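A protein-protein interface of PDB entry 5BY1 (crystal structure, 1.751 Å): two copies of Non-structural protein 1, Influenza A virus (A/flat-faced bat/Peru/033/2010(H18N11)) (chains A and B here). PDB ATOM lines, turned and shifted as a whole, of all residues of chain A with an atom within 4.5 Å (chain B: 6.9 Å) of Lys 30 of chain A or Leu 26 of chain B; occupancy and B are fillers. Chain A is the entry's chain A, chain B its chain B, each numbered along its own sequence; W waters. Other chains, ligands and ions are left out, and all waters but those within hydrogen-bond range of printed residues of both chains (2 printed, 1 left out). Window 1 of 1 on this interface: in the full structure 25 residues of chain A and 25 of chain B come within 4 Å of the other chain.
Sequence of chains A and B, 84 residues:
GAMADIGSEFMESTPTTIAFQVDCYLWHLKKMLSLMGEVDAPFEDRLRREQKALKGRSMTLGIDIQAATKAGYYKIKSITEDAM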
ATOM      1  N   LEU A  26     -19.757 -22.950  -4.743  1.00  0.00           N
ATOM      2  CA  LEU A  26     -20.512 -23.373  -3.562  1.00  0.00           C
ATOM      3  C   LEU A  26     -19.837 -22.853  -2.284  1.00  0.00           C
ATOM      4  O   LEU A  26     -20.512 -22.538  -1.311  1.00  0.00           O
ATOM      5  CB  LEU A  26     -20.680 -24.896  -3.530  1.00  0.00           C
ATOM      6  CG  LEU A  26     -21.520 -25.397  -4.700  1.00  0.00           C
ATOM      7  CD1 LEU A  26     -21.865 -26.876  -4.511  1.00  0.00           C
ATOM      8  CD2 LEU A  26     -22.789 -24.565  -4.925  1.00  0.00           C
ATOM      9  N   TRP A  27     -18.514 -22.709  -2.300  1.00  0.00           N
ATOM     10  CA  TRP A  27     -17.818 -22.125  -1.157  1.00  0.00           C
ATOM     11  C   TRP A  27     -18.264 -20.679  -0.957  1.00  0.00           C
ATOM     12  O   TRP A  27     -18.469 -20.227   0.173  1.00  0.00           O
ATOM     13  CB  TRP A  27     -16.298 -22.179  -1.339  1.00  0.00           C
ATOM     14  CG  TRP A  27     -15.541 -21.534  -0.204  1.00  0.00           C
ATOM     15  CD1 TRP A  27     -15.100 -22.139   0.940  1.00  0.00           C
ATOM     16  CD2 TRP A  27     -15.161 -20.158  -0.098  1.00  0.00           C
ATOM     17  NE1 TRP A  27     -14.465 -21.220   1.749  1.00  0.00           N
ATOM     18  CE2 TRP A  27     -14.492 -19.999   1.132  1.00  0.00           C
ATOM     19  CE3 TRP A  27     -15.337 -19.038  -0.919  1.00  0.00           C
ATOM     20  CZ2 TRP A  27     -13.988 -18.774   1.554  1.00  0.00           C
ATOM     21  CZ3 TRP A  27     -14.828 -17.823  -0.499  1.00  0.00           C
ATOM     22  CH2 TRP A  27     -14.169 -17.700   0.725  1.00  0.00           C
ATOM     23  N   HIS A  28     -18.379 -19.950  -2.063  1.00  0.00           N
ATOM     24  CA  HIS A  28     -18.889 -18.575  -2.047  1.00  0.00           C
ATOM     25  C   HIS A  28     -20.259 -18.475  -1.370  1.00  0.00           C
ATOM     26  O   HIS A  28     -20.524 -17.534  -0.621  1.00  0.00           O
ATOM     27  CB  HIS A  28     -18.983 -18.011  -3.470  1.00  0.00           C
ATOM     28  CG  HIS A  28     -19.510 -16.614  -3.518  1.00  0.00           C
ATOM     29  ND1 HIS A  28     -18.712 -15.513  -3.287  1.00  0.00           N
ATOM     30  CD2 HIS A  28     -20.764 -16.136  -3.700  1.00  0.00           C
ATOM     31  CE1 HIS A  28     -19.445 -14.419  -3.352  1.00  0.00           C
ATOM     32  NE2 HIS A  28     -20.697 -14.770  -3.595  1.00  0.00           N
ATOM     33  N   LEU A  29     -21.132 -19.439  -1.629  1.00  0.00           N
ATOM     34  CA  LEU A  29     -22.450 -19.427  -1.017  1.00  0.00           C
ATOM     35  C   LEU A  29     -22.347 -19.637   0.495  1.00  0.00           C
ATOM     36  O   LEU A  29     -23.065 -18.986   1.271  1.00  0.00           O
ATOM     37  CB  LEU A  29     -23.343 -20.502  -1.660  1.00  0.00           C
ATOM     38  CG  LEU A  29     -23.811 -20.256  -3.098  1.00  0.00           C
ATOM     39  CD1 LEU A  29     -24.636 -21.437  -3.620  1.00  0.00           C
ATOM     40  CD2 LEU A  29     -24.617 -18.966  -3.200  1.00  0.00           C
ATOM     41  N   LYS A  30     -21.451 -20.521   0.918  1.00  0.00           N
ATOM     42  CA  LYS A  30     -21.196 -20.703   2.341  1.00  0.00           C
ATOM     43  C   LYS A  30     -20.620 -19.433   2.956  1.00  0.00           C
ATOM     44  O   LYS A  30     -20.923 -19.088   4.103  1.00  0.00           O
ATOM     45  CB  LYS A  30     -20.247 -21.874   2.585  1.00  0.00           C
ATOM     46  CG  LYS A  30     -20.900 -23.201   2.218  1.00  0.00           C
ATOM     47  CD  LYS A  30     -20.159 -24.406   2.779  1.00  0.00           C
ATOM     48  CE  LYS A  30     -21.011 -25.666   2.545  1.00  0.00           C
ATOM     49  NZ  LYS A  30     -20.347 -26.963   2.935  1.00  0.00           N
ATOM     50  N   LYS A  31     -19.803 -18.719   2.187  1.00  0.00           N
ATOM     51  CA  LYS A  31     -19.267 -17.459   2.701  1.00  0.00           C
ATOM     52  C   LYS A  31     -20.404 -16.466   2.909  1.00  0.00           C
ATOM     53  O   LYS A  31     -20.416 -15.725   3.884  1.00  0.00           O
ATOM     54  CB  LYS A  31     -18.193 -16.875   1.764  1.00  0.00           C
ATOM     55  CG  LYS A  31     -17.621 -15.533   2.266  1.00  0.00           C
ATOM     56  CD  LYS A  31     -16.500 -14.992   1.392  1.00  0.00           C
ATOM     57  CE  LYS A  31     -16.980 -14.650  -0.013  1.00  0.00           C
ATOM     58  NZ  LYS A  31     -18.004 -13.582  -0.023  1.00  0.00           N
ATOM     59  N   MET A  32     -21.375 -16.452   2.003  1.00  0.00           N
ATOM     60  CA  MET A  32     -22.481 -15.523   2.143  1.00  0.00           C
ATOM     61  C   MET A  32     -23.250 -15.767   3.450  1.00  0.00           C
ATOM     62  O   MET A  32     -23.668 -14.808   4.117  1.00  0.00           O
ATOM     63  CB  MET A  32     -23.399 -15.624   0.935  1.00  0.00           C
ATOM     64  CG  MET A  32     -22.768 -15.032  -0.320  1.00  0.00           C
ATOM     65  SD  MET A  32     -23.843 -15.216  -1.760  1.00  0.00           S
ATOM     66  CE  MET A  32     -24.982 -13.844  -1.528  1.00  0.00           C
ATOM     67  N   LEU A  33     -23.422 -17.038   3.819  1.00  0.00           N
ATOM     68  CA  LEU A  33     -24.042 -17.397   5.106  1.00  0.00           C
ATOM     69  C   LEU A  33     -23.222 -16.894   6.290  1.00  0.00           C
ATOM     70  O   LEU A  33     -23.769 -16.404   7.272  1.00  0.00           O
ATOM     71  CB  LEU A  33     -24.217 -18.914   5.230  1.00  0.00           C
ATOM     72  CG  LEU A  33     -25.555 -19.538   4.822  1.00  0.00           C
ATOM     73  CD1 LEU A  33     -26.716 -19.053   5.707  1.00  0.00           C
ATOM     74  CD2 LEU A  33     -25.843 -19.261   3.360  1.00  0.00           C
ATOM     75  N   SER A  34     -21.904 -17.034   6.207  1.00  0.00           N
ATOM     76  CA  SER A  34     -21.024 -16.450   7.211  1.00  0.00           C
ATOM     77  C   SER A  34     -21.200 -14.932   7.306  1.00  0.00           C
ATOM     78  O   SER A  34     -21.251 -14.379   8.411  1.00  0.00           O
ATOM     79  CB  SER A  34     -19.570 -16.791   6.899  1.00  0.00           C
ATOM     80  OG  SER A  34     -18.719 -16.244   7.881  1.00  0.00           O
ATOM     81  N   PHE A  43     -18.860 -24.341  11.366  1.00  0.00           N
ATOM     82  CA  PHE A  43     -19.125 -23.974   9.967  1.00  0.00           C
ATOM     83  C   PHE A  43     -18.083 -22.962   9.481  1.00  0.00           C
ATOM     84  O   PHE A  43     -17.543 -23.100   8.387  1.00  0.00           O
ATOM     85  CB  PHE A  43     -20.549 -23.414   9.818  1.00  0.00           C
ATOM     86  CG  PHE A  43     -20.936 -23.061   8.392  1.00  0.00           C
ATOM     87  CD1 PHE A  43     -20.556 -21.846   7.830  1.00  0.00           C
ATOM     88  CD2 PHE A  43     -21.689 -23.933   7.626  1.00  0.00           C
ATOM     89  CE1 PHE A  43     -20.913 -21.513   6.520  1.00  0.00           C
ATOM     90  CE2 PHE A  43     -22.049 -23.611   6.320  1.00  0.00           C
ATOM     91  CZ  PHE A  43     -21.659 -22.396   5.770  1.00  0.00           C
ATOM     92  N   LEU A  47     -15.139 -23.334   6.654  1.00  0.00           N
ATOM     93  CA  LEU A  47     -15.035 -22.310   5.617  1.00  0.00           C
ATOM     94  C   LEU A  47     -13.587 -21.864   5.413  1.00  0.00           C
ATOM     95  O   LEU A  47     -13.122 -21.759   4.272  1.00  0.00           O
ATOM     96  CB  LEU A  47     -15.915 -21.102   5.970  1.00  0.00           C
ATOM     97  CG  LEU A  47     -16.065 -20.019   4.889  1.00  0.00           C
ATOM     98  CD1 LEU A  47     -17.004 -20.499   3.781  1.00  0.00           C
ATOM     99  CD2 LEU A  47     -16.538 -18.658   5.464  1.00  0.00           C
ATOM    100  N   ALA B  19     -26.568 -24.001   9.648  1.00  0.00           N
ATOM    101  CA  ALA B  19     -25.329 -24.526   9.068  1.00  0.00           C
ATOM    102  C   ALA B  19     -25.548 -25.931   8.503  1.00  0.00           C
ATOM    103  O   ALA B  19     -25.098 -26.230   7.402  1.00  0.00           O
ATOM    104  CB  ALA B  19     -24.205 -24.536  10.104  1.00  0.00           C
ATOM    105  N   PHE B  20     -26.242 -26.778   9.263  1.00  0.00           N
ATOM    106  CA  PHE B  20     -26.544 -28.144   8.821  1.00  0.00           C
ATOM    107  C   PHE B  20     -27.410 -28.160   7.563  1.00  0.00           C
ATOM    108  O   PHE B  20     -27.107 -28.866   6.605  1.00  0.00           O
ATOM    109  CB  PHE B  20     -27.232 -28.927   9.943  1.00  0.00           C
ATOM    110  CG  PHE B  20     -27.433 -30.392   9.631  1.00  0.00           C
ATOM    111  CD1 PHE B  20     -26.344 -31.224   9.403  1.00  0.00           C
ATOM    112  CD2 PHE B  20     -28.698 -30.931   9.575  1.00  0.00           C
ATOM    113  CE1 PHE B  20     -26.521 -32.564   9.130  1.00  0.00           C
ATOM    114  CE2 PHE B  20     -28.883 -32.280   9.281  1.00  0.00           C
ATOM    115  CZ  PHE B  20     -27.793 -33.089   9.061  1.00  0.00           C
ATOM    116  N   GLN B  21     -28.483 -27.381   7.571  1.00  0.00           N
ATOM    117  CA  GLN B  21     -29.383 -27.295   6.429  1.00  0.00           C
ATOM    118  C   GLN B  21     -28.632 -26.868   5.170  1.00  0.00           C
ATOM    119  O   GLN B  21     -28.760 -27.490   4.119  1.00  0.00           O
ATOM    120  CB  GLN B  21     -30.526 -26.321   6.731  1.00  0.00           C
ATOM    121  CG  GLN B  21     -31.439 -26.817   7.857  1.00  0.00           C
ATOM    122  CD  GLN B  21     -32.378 -25.744   8.379  1.00  0.00           C
ATOM    123  OE1 GLN B  21     -32.186 -24.561   8.119  1.00  0.00           O
ATOM    124  NE2 GLN B  21     -33.406 -26.156   9.109  1.00  0.00           N
ATOM    125  N   VAL B  22     -27.827 -25.818   5.287  1.00  0.00           N
ATOM    126  CA  VAL B  22     -27.065 -25.336   4.144  1.00  0.00           C
ATOM    127  C   VAL B  22     -26.030 -26.368   3.697  1.00  0.00           C
ATOM    128  O   VAL B  22     -25.878 -26.612   2.501  1.00  0.00           O
ATOM    129  CB  VAL B  22     -26.374 -23.996   4.455  1.00  0.00           C
ATOM    130  CG1 VAL B  22     -25.354 -23.651   3.364  1.00  0.00           C
ATOM    131  CG2 VAL B  22     -27.430 -22.899   4.590  1.00  0.00           C
ATOM    132  N   ASP B  23     -25.327 -26.987   4.644  1.00  0.00           N
ATOM    133  CA  ASP B  23     -24.356 -28.029   4.287  1.00  0.00           C
ATOM    134  C   ASP B  23     -25.026 -29.180   3.539  1.00  0.00           C
ATOM    135  O   ASP B  23     -24.466 -29.709   2.578  1.00  0.00           O
ATOM    136  CB  ASP B  23     -23.653 -28.589   5.524  1.00  0.00           C
ATOM    137  CG  ASP B  23     -22.589 -27.662   6.070  1.00  0.00           C
ATOM    138  OD1 ASP B  23     -22.118 -26.773   5.329  1.00  0.00           O
ATOM    139  OD2 ASP B  23     -22.195 -27.856   7.236  1.00  0.00           O
ATOM    140  N   CYS B  24     -26.224 -29.564   3.982  1.00  0.00           N
ATOM    141  CA  CYS B  24     -26.928 -30.689   3.361  1.00  0.00           C
ATOM    142  C   CYS B  24     -27.323 -30.367   1.946  1.00  0.00           C
ATOM    143  O   CYS B  24     -27.151 -31.180   1.044  1.00  0.00           O
ATOM    144  CB  CYS B  24     -28.175 -31.080   4.153  1.00  0.00           C
ATOM    145  SG  CYS B  24     -27.819 -32.036   5.638  1.00  0.00           S
ATOM    146  N   TYR B  25     -27.868 -29.178   1.745  1.00  0.00           N
ATOM    147  CA  TYR B  25     -28.300 -28.813   0.408  1.00  0.00           C
ATOM    148  C   TYR B  25     -27.118 -28.684  -0.560  1.00  0.00           C
ATOM    149  O   TYR B  25     -27.178 -29.154  -1.701  1.00  0.00           O
ATOM    150  CB  TYR B  25     -29.114 -27.509   0.427  1.00  0.00           C
ATOM    151  CG  TYR B  25     -29.459 -27.083  -0.987  1.00  0.00           C
ATOM    152  CD1 TYR B  25     -30.259 -27.886  -1.786  1.00  0.00           C
ATOM    153  CD2 TYR B  25     -28.947 -25.916  -1.532  1.00  0.00           C
ATOM    154  CE1 TYR B  25     -30.552 -27.531  -3.078  1.00  0.00           C
ATOM    155  CE2 TYR B  25     -29.240 -25.550  -2.838  1.00  0.00           C
ATOM    156  CZ  TYR B  25     -30.040 -26.370  -3.601  1.00  0.00           C
ATOM    157  OH  TYR B  25     -30.341 -26.023  -4.899  1.00  0.00           O
ATOM    158  N   LEU B  26     -26.027 -28.059  -0.122  1.00  0.00           N
ATOM    159  CA  LEU B  26     -24.924 -27.868  -1.038  1.00  0.00           C
ATOM    160  C   LEU B  26     -24.256 -29.215  -1.328  1.00  0.00           C
ATOM    161  O   LEU B  26     -23.799 -29.471  -2.445  1.00  0.00           O
ATOM    162  CB  LEU B  26     -23.940 -26.836  -0.467  1.00  0.00           C
ATOM    163  CG  LEU B  26     -24.583 -25.452  -0.292  1.00  0.00           C
ATOM    164  CD1 LEU B  26     -23.565 -24.427   0.210  1.00  0.00           C
ATOM    165  CD2 LEU B  26     -25.221 -24.946  -1.600  1.00  0.00           C
ATOM    166  N   TRP B  27     -24.252 -30.099  -0.335  1.00  0.00           N
ATOM    167  CA  TRP B  27     -23.783 -31.451  -0.554  1.00  0.00           C
ATOM    168  C   TRP B  27     -24.655 -32.162  -1.591  1.00  0.00           C
ATOM    169  O   TRP B  27     -24.149 -32.887  -2.449  1.00  0.00           O
ATOM    170  CB  TRP B  27     -23.772 -32.249   0.753  1.00  0.00           C
ATOM    171  CG  TRP B  27     -23.356 -33.652   0.518  1.00  0.00           C
ATOM    172  CD1 TRP B  27     -22.076 -34.127   0.421  1.00  0.00           C
ATOM    173  CD2 TRP B  27     -24.220 -34.775   0.300  1.00  0.00           C
ATOM    174  NE1 TRP B  27     -22.097 -35.479   0.171  1.00  0.00           N
ATOM    175  CE2 TRP B  27     -23.400 -35.897   0.087  1.00  0.00           C
ATOM    176  CE3 TRP B  27     -25.610 -34.937   0.265  1.00  0.00           C
ATOM    177  CZ2 TRP B  27     -23.924 -37.164  -0.165  1.00  0.00           C
ATOM    178  CZ3 TRP B  27     -26.126 -36.194   0.025  1.00  0.00           C
ATOM    179  CH2 TRP B  27     -25.284 -37.292  -0.180  1.00  0.00           C
ATOM    180  N   HIS B  28     -25.968 -31.957  -1.494  1.00  0.00           N
ATOM    181  CA  HIS B  28     -26.917 -32.553  -2.428  1.00  0.00           C
ATOM    182  C   HIS B  28     -26.601 -32.125  -3.868  1.00  0.00           C
ATOM    183  O   HIS B  28     -26.626 -32.941  -4.797  1.00  0.00           O
ATOM    184  CB  HIS B  28     -28.337 -32.160  -2.027  1.00  0.00           C
ATOM    185  CG  HIS B  28     -29.346 -32.322  -3.117  1.00  0.00           C
ATOM    186  ND1 HIS B  28     -29.854 -33.547  -3.490  1.00  0.00           N
ATOM    187  CD2 HIS B  28     -29.960 -31.403  -3.902  1.00  0.00           C
ATOM    188  CE1 HIS B  28     -30.723 -33.377  -4.471  1.00  0.00           C
ATOM    189  NE2 HIS B  28     -30.812 -32.086  -4.733  1.00  0.00           N
ATOM    190  N   LEU B  29     -26.277 -30.850  -4.047  1.00  0.00           N
ATOM    191  CA  LEU B  29     -25.851 -30.358  -5.355  1.00  0.00           C
ATOM    192  C   LEU B  29     -24.584 -31.053  -5.817  1.00  0.00           C
ATOM    193  O   LEU B  29     -24.491 -31.467  -6.974  1.00  0.00           O
ATOM    194  CB  LEU B  29     -25.619 -28.853  -5.330  1.00  0.00           C
ATOM    195  CG  LEU B  29     -26.893 -28.020  -5.165  1.00  0.00           C
ATOM    196  CD1 LEU B  29     -26.572 -26.541  -5.256  1.00  0.00           C
ATOM    197  CD2 LEU B  29     -27.928 -28.419  -6.222  1.00  0.00           C
ATOM    198  N   LYS B  30     -23.596 -31.161  -4.930  1.00  0.00           N
ATOM    199  CA  LYS B  30     -22.359 -31.838  -5.314  1.00  0.00           C
ATOM    200  C   LYS B  30     -22.626 -33.311  -5.686  1.00  0.00           C
ATOM    201  O   LYS B  30     -22.054 -33.829  -6.644  1.00  0.00           O
ATOM    202  CB  LYS B  30     -21.327 -31.738  -4.202  1.00  0.00           C
ATOM    203  CG  LYS B  30     -20.864 -30.301  -3.984  1.00  0.00           C
ATOM    204  CD  LYS B  30     -19.607 -30.209  -3.149  1.00  0.00           C
ATOM    205  CE  LYS B  30     -19.137 -28.745  -3.123  1.00  0.00           C
ATOM    206  NZ  LYS B  30     -17.883 -28.530  -2.343  1.00  0.00           N
ATOM    207  N   LYS B  31     -23.511 -33.973  -4.944  1.00  0.00           N
ATOM    208  CA  LYS B  31     -23.829 -35.363  -5.246  1.00  0.00           C
ATOM    209  C   LYS B  31     -24.457 -35.490  -6.628  1.00  0.00           C
ATOM    210  O   LYS B  31     -24.124 -36.378  -7.412  1.00  0.00           O
ATOM    211  CB  LYS B  31     -24.777 -35.950  -4.204  1.00  0.00           C
ATOM    212  CG  LYS B  31     -25.252 -37.347  -4.575  1.00  0.00           C
ATOM    213  CD  LYS B  31     -26.326 -37.835  -3.634  1.00  0.00           C
ATOM    214  CE  LYS B  31     -27.623 -37.109  -3.888  1.00  0.00           C
ATOM    215  NZ  LYS B  31     -28.654 -37.521  -2.908  1.00  0.00           N
ATOM    216  N   PHE B  43     -13.091 -34.961  -6.195  1.00  0.00           N
ATOM    217  CA  PHE B  43     -14.364 -34.316  -5.849  1.00  0.00           C
ATOM    218  C   PHE B  43     -15.321 -35.380  -5.282  1.00  0.00           C
ATOM    219  O   PHE B  43     -16.024 -35.145  -4.294  1.00  0.00           O
ATOM    220  CB  PHE B  43     -14.948 -33.622  -7.093  1.00  0.00           C
ATOM    221  CG  PHE B  43     -16.255 -32.874  -6.865  1.00  0.00           C
ATOM    222  CD1 PHE B  43     -17.456 -33.566  -6.788  1.00  0.00           C
ATOM    223  CD2 PHE B  43     -16.288 -31.482  -6.806  1.00  0.00           C
ATOM    224  CE1 PHE B  43     -18.659 -32.909  -6.629  1.00  0.00           C
ATOM    225  CE2 PHE B  43     -17.504 -30.804  -6.644  1.00  0.00           C
ATOM    226  CZ  PHE B  43     -18.696 -31.530  -6.553  1.00  0.00           C
ATOM    227  N   LEU B  47     -16.850 -35.725  -1.590  1.00  0.00           N
ATOM    228  CA  LEU B  47     -18.287 -35.939  -1.461  1.00  0.00           C
ATOM    229  C   LEU B  47     -18.652 -37.020  -0.436  1.00  0.00           C
ATOM    230  O   LEU B  47     -19.508 -36.816   0.420  1.00  0.00           O
ATOM    231  CB  LEU B  47     -18.876 -36.319  -2.811  1.00  0.00           C
ATOM    232  CG  LEU B  47     -20.393 -36.450  -2.778  1.00  0.00           C
ATOM    233  CD1 LEU B  47     -21.050 -35.054  -2.849  1.00  0.00           C
ATOM    234  CD2 LEU B  47     -20.878 -37.332  -3.894  1.00  0.00           C
ATOM    235  N   GLU B  50     -17.725 -36.055   3.168  1.00  0.00           N
ATOM    236  CA  GLU B  50     -18.687 -35.109   3.731  1.00  0.00           C
ATOM    237  C   GLU B  50     -19.992 -35.790   4.123  1.00  0.00           C
ATOM    238  O   GLU B  50     -20.565 -35.488   5.163  1.00  0.00           O
ATOM    239  CB  GLU B  50     -18.992 -33.974   2.753  1.00  0.00           C
ATOM    240  CG  GLU B  50     -19.847 -32.857   3.391  1.00  0.00           C
ATOM    241  CD  GLU B  50     -19.998 -31.629   2.502  1.00  0.00           C
ATOM    242  OE1 GLU B  50     -19.577 -31.685   1.323  1.00  0.00           O
ATOM    243  OE2 GLU B  50     -20.530 -30.599   2.990  1.00  0.00           O
ATOM    244  N   ARG B  57     -23.535 -35.744  12.117  1.00  0.00           N
ATOM    245  CA  ARG B  57     -24.178 -34.528  12.606  1.00  0.00           C
ATOM    246  C   ARG B  57     -25.697 -34.676  12.695  1.00  0.00           C
ATOM    247  O   ARG B  57     -26.326 -34.154  13.618  1.00  0.00           O
ATOM    248  CB  ARG B  57     -23.813 -33.340  11.712  1.00  0.00           C
ATOM    249  CG  ARG B  57     -22.371 -32.891  11.893  1.00  0.00           C
ATOM    250  CD  ARG B  57     -21.878 -32.027  10.746  1.00  0.00           C
ATOM    251  NE  ARG B  57     -22.618 -30.781  10.649  1.00  0.00           N
ATOM    252  CZ  ARG B  57     -22.532 -29.950   9.615  1.00  0.00           C
ATOM    253  NH1 ARG B  57     -21.734 -30.258   8.606  1.00  0.00           N
ATOM    254  NH2 ARG B  57     -23.247 -28.829   9.594  1.00  0.00           N
ATOM    255  N   THR B  69     -32.016 -30.861   3.803  1.00  0.00           N
ATOM    256  CA  THR B  69     -31.679 -30.522   2.428  1.00  0.00           C
ATOM    257  C   THR B  69     -32.728 -29.556   1.861  1.00  0.00           C
ATOM    258  O   THR B  69     -32.397 -28.547   1.229  1.00  0.00           O
ATOM    259  CB  THR B  69     -31.581 -31.787   1.542  1.00  0.00           C
ATOM    260  OG1 THR B  69     -30.567 -32.656   2.068  1.00  0.00           O
ATOM    261  CG2 THR B  69     -31.204 -31.390   0.109  1.00  0.00           C
ATOM    262  N   GLY B  72     -32.364 -26.163   3.479  1.00  0.00           N
ATOM    263  CA  GLY B  72     -31.161 -25.518   2.976  1.00  0.00           C
ATOM    264  C   GLY B  72     -31.367 -24.953   1.583  1.00  0.00           C
ATOM    265  O   GLY B  72     -30.803 -23.916   1.227  1.00  0.00           O
ATOM    266  N   TYR B  73     -32.185 -25.629   0.787  1.00  0.00           N
ATOM    267  CA  TYR B  73     -32.531 -25.112  -0.526  1.00  0.00           C
ATOM    268  C   TYR B  73     -33.235 -23.757  -0.408  1.00  0.00           C
ATOM    269  O   TYR B  73     -32.951 -22.827  -1.161  1.00  0.00           O
ATOM    270  CB  TYR B  73     -33.408 -26.111  -1.266  1.00  0.00           C
ATOM    271  CG  TYR B  73     -34.114 -25.541  -2.478  1.00  0.00           C
ATOM    272  CD1 TYR B  73     -33.504 -25.544  -3.728  1.00  0.00           C
ATOM    273  CD2 TYR B  73     -35.388 -24.993  -2.370  1.00  0.00           C
ATOM    274  CE1 TYR B  73     -34.150 -25.030  -4.839  1.00  0.00           C
ATOM    275  CE2 TYR B  73     -36.038 -24.467  -3.474  1.00  0.00           C
ATOM    276  CZ  TYR B  73     -35.416 -24.492  -4.703  1.00  0.00           C
ATOM    277  OH  TYR B  73     -36.063 -23.973  -5.806  1.00  0.00           O
ATOM    278  N   ILE B  76     -30.768 -20.983   0.806  1.00  0.00           N
ATOM    279  CA  ILE B  76     -29.939 -20.539  -0.311  1.00  0.00           C
ATOM    280  C   ILE B  76     -30.747 -19.722  -1.330  1.00  0.00           C
ATOM    281  O   ILE B  76     -30.291 -18.681  -1.796  1.00  0.00           O
ATOM    282  CB  ILE B  76     -29.263 -21.728  -1.014  1.00  0.00           C
ATOM    283  CG1 ILE B  76     -28.198 -22.339  -0.098  1.00  0.00           C
ATOM    284  CG2 ILE B  76     -28.612 -21.294  -2.320  1.00  0.00           C
ATOM    285  CD1 ILE B  76     -27.110 -21.350   0.319  1.00  0.00           C
ATOM    286  N   ILE B  79     -31.116 -16.206  -0.096  1.00  0.00           N
ATOM    287  CA  ILE B  79     -29.928 -15.359  -0.060  1.00  0.00           C
ATOM    288  C   ILE B  79     -29.431 -14.980  -1.452  1.00  0.00           C
ATOM    289  O   ILE B  79     -28.842 -13.915  -1.636  1.00  0.00           O
ATOM    290  CB  ILE B  79     -28.775 -16.034   0.723  1.00  0.00           C
ATOM    291  CG1 ILE B  79     -28.266 -17.285   0.005  1.00  0.00           C
ATOM    292  CG2 ILE B  79     -29.238 -16.411   2.114  1.00  0.00           C
ATOM    293  CD1 ILE B  79     -26.786 -17.251  -0.331  1.00  0.00           C
HETATM  294  O   HOH W   1     -19.567 -26.173   6.091  1.00  0.00           O
HETATM  295  O   HOH W   2     -17.311 -25.880  -1.911  1.00  0.00           O
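Lys 30 of chain A touches just these residues of chain B: Asp 23, Leu 26 and Glu 50.
Leu 26 of chain B touches two residues of chain A.
Printed residues of chain A within 4 Å of Ile 79 of chain B: Leu 29 and Met 32.
Of the printed residues of chain A, Ile 76 of chain B touches Leu 33 (3.9 Å).
The nearest printed residue of chain B that does not touch Phe 43 of chain A is Val 22 of chain B (4.4 Å).
Of the 11 printed residues of chain A, 6 touch a printed residue of chain B.
Hydrophobic or aromatic side chains of chain B that line the printed part of chain A: Ala 19, Val 22, Leu 26, Ile 76 and Ile 79.
Among the printed residues, 11 pairs touch across the chains.
NZ of Lys 30 of chain A is in salt-bridge range of OE2 of Glu 50 of chain B (3.6 Å).
NZ of Lys 30 of chain A is in salt-bridge range of OD1 of Asp 23 of chain B, 3.0 Å away.
Leu 26 of chain A touches Leu 26 of chain B (CD1 to O, 3.8 Å).
CE of Lys 30 of chain B touches CD1 of Leu 26 of chain A, 3.6 Å away.
CD2 of Leu 29 of chain A touches CD1 of Ile 79 of chain B (3.98 Å).
Lys 30 of chain A touches Leu 26 of chain B.
Ile 79 of chain B touches Met 32 of chain A.
Val 22 of chain B touches Leu 33 of chain A.
Leu 33 of chain A touches Ile 76 of chain B (CD2 to CD1, 3.9 Å).
CD2 of Phe 43 of chain A touches CB of Ala 19 of chain B, at 3.6 Å.
Phe 43 of chain A touches Asp 23 of chain B.
Water W1 lies within hydrogen-bond range of the side-chain carboxylate (OD1) of Asp 23 of chain B and the side-chain amino group (NZ) of Lys 30 of chain A.
Water W2 lies within hydrogen-bond range of the side-chain amino group (NZ) of Lys 30 of chain B (2.7 Å) and the backbone NH (N) of Trp 27 of chain A (3.4 Å).
Leu 26 of chain A touches its own counterpart, Leu 26 of chain B.
Leu 26 of chain A touches Lys 30 of chain B, and with the chains exchanged Lys 30 of chain A touches Leu 26 of chain B.
Positions printed for both chains: 26, 27, 28, 29, 30, 31, 43 and 47.
Of the 11 pairs that touch across the chains among the printed residues, 3 have their exchanged pair printed and touching as well.
A ring nitrogen (NE2) of His 28 of chain A is in hydrogen-bond range of the side-chain sulfur (SD) of Met 32 of chain A, at 3.7 Å.
OD2 of Asp 23 of chain B is in salt-bridge range of NH2 of Arg 57 of chain B (2.8 Å).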
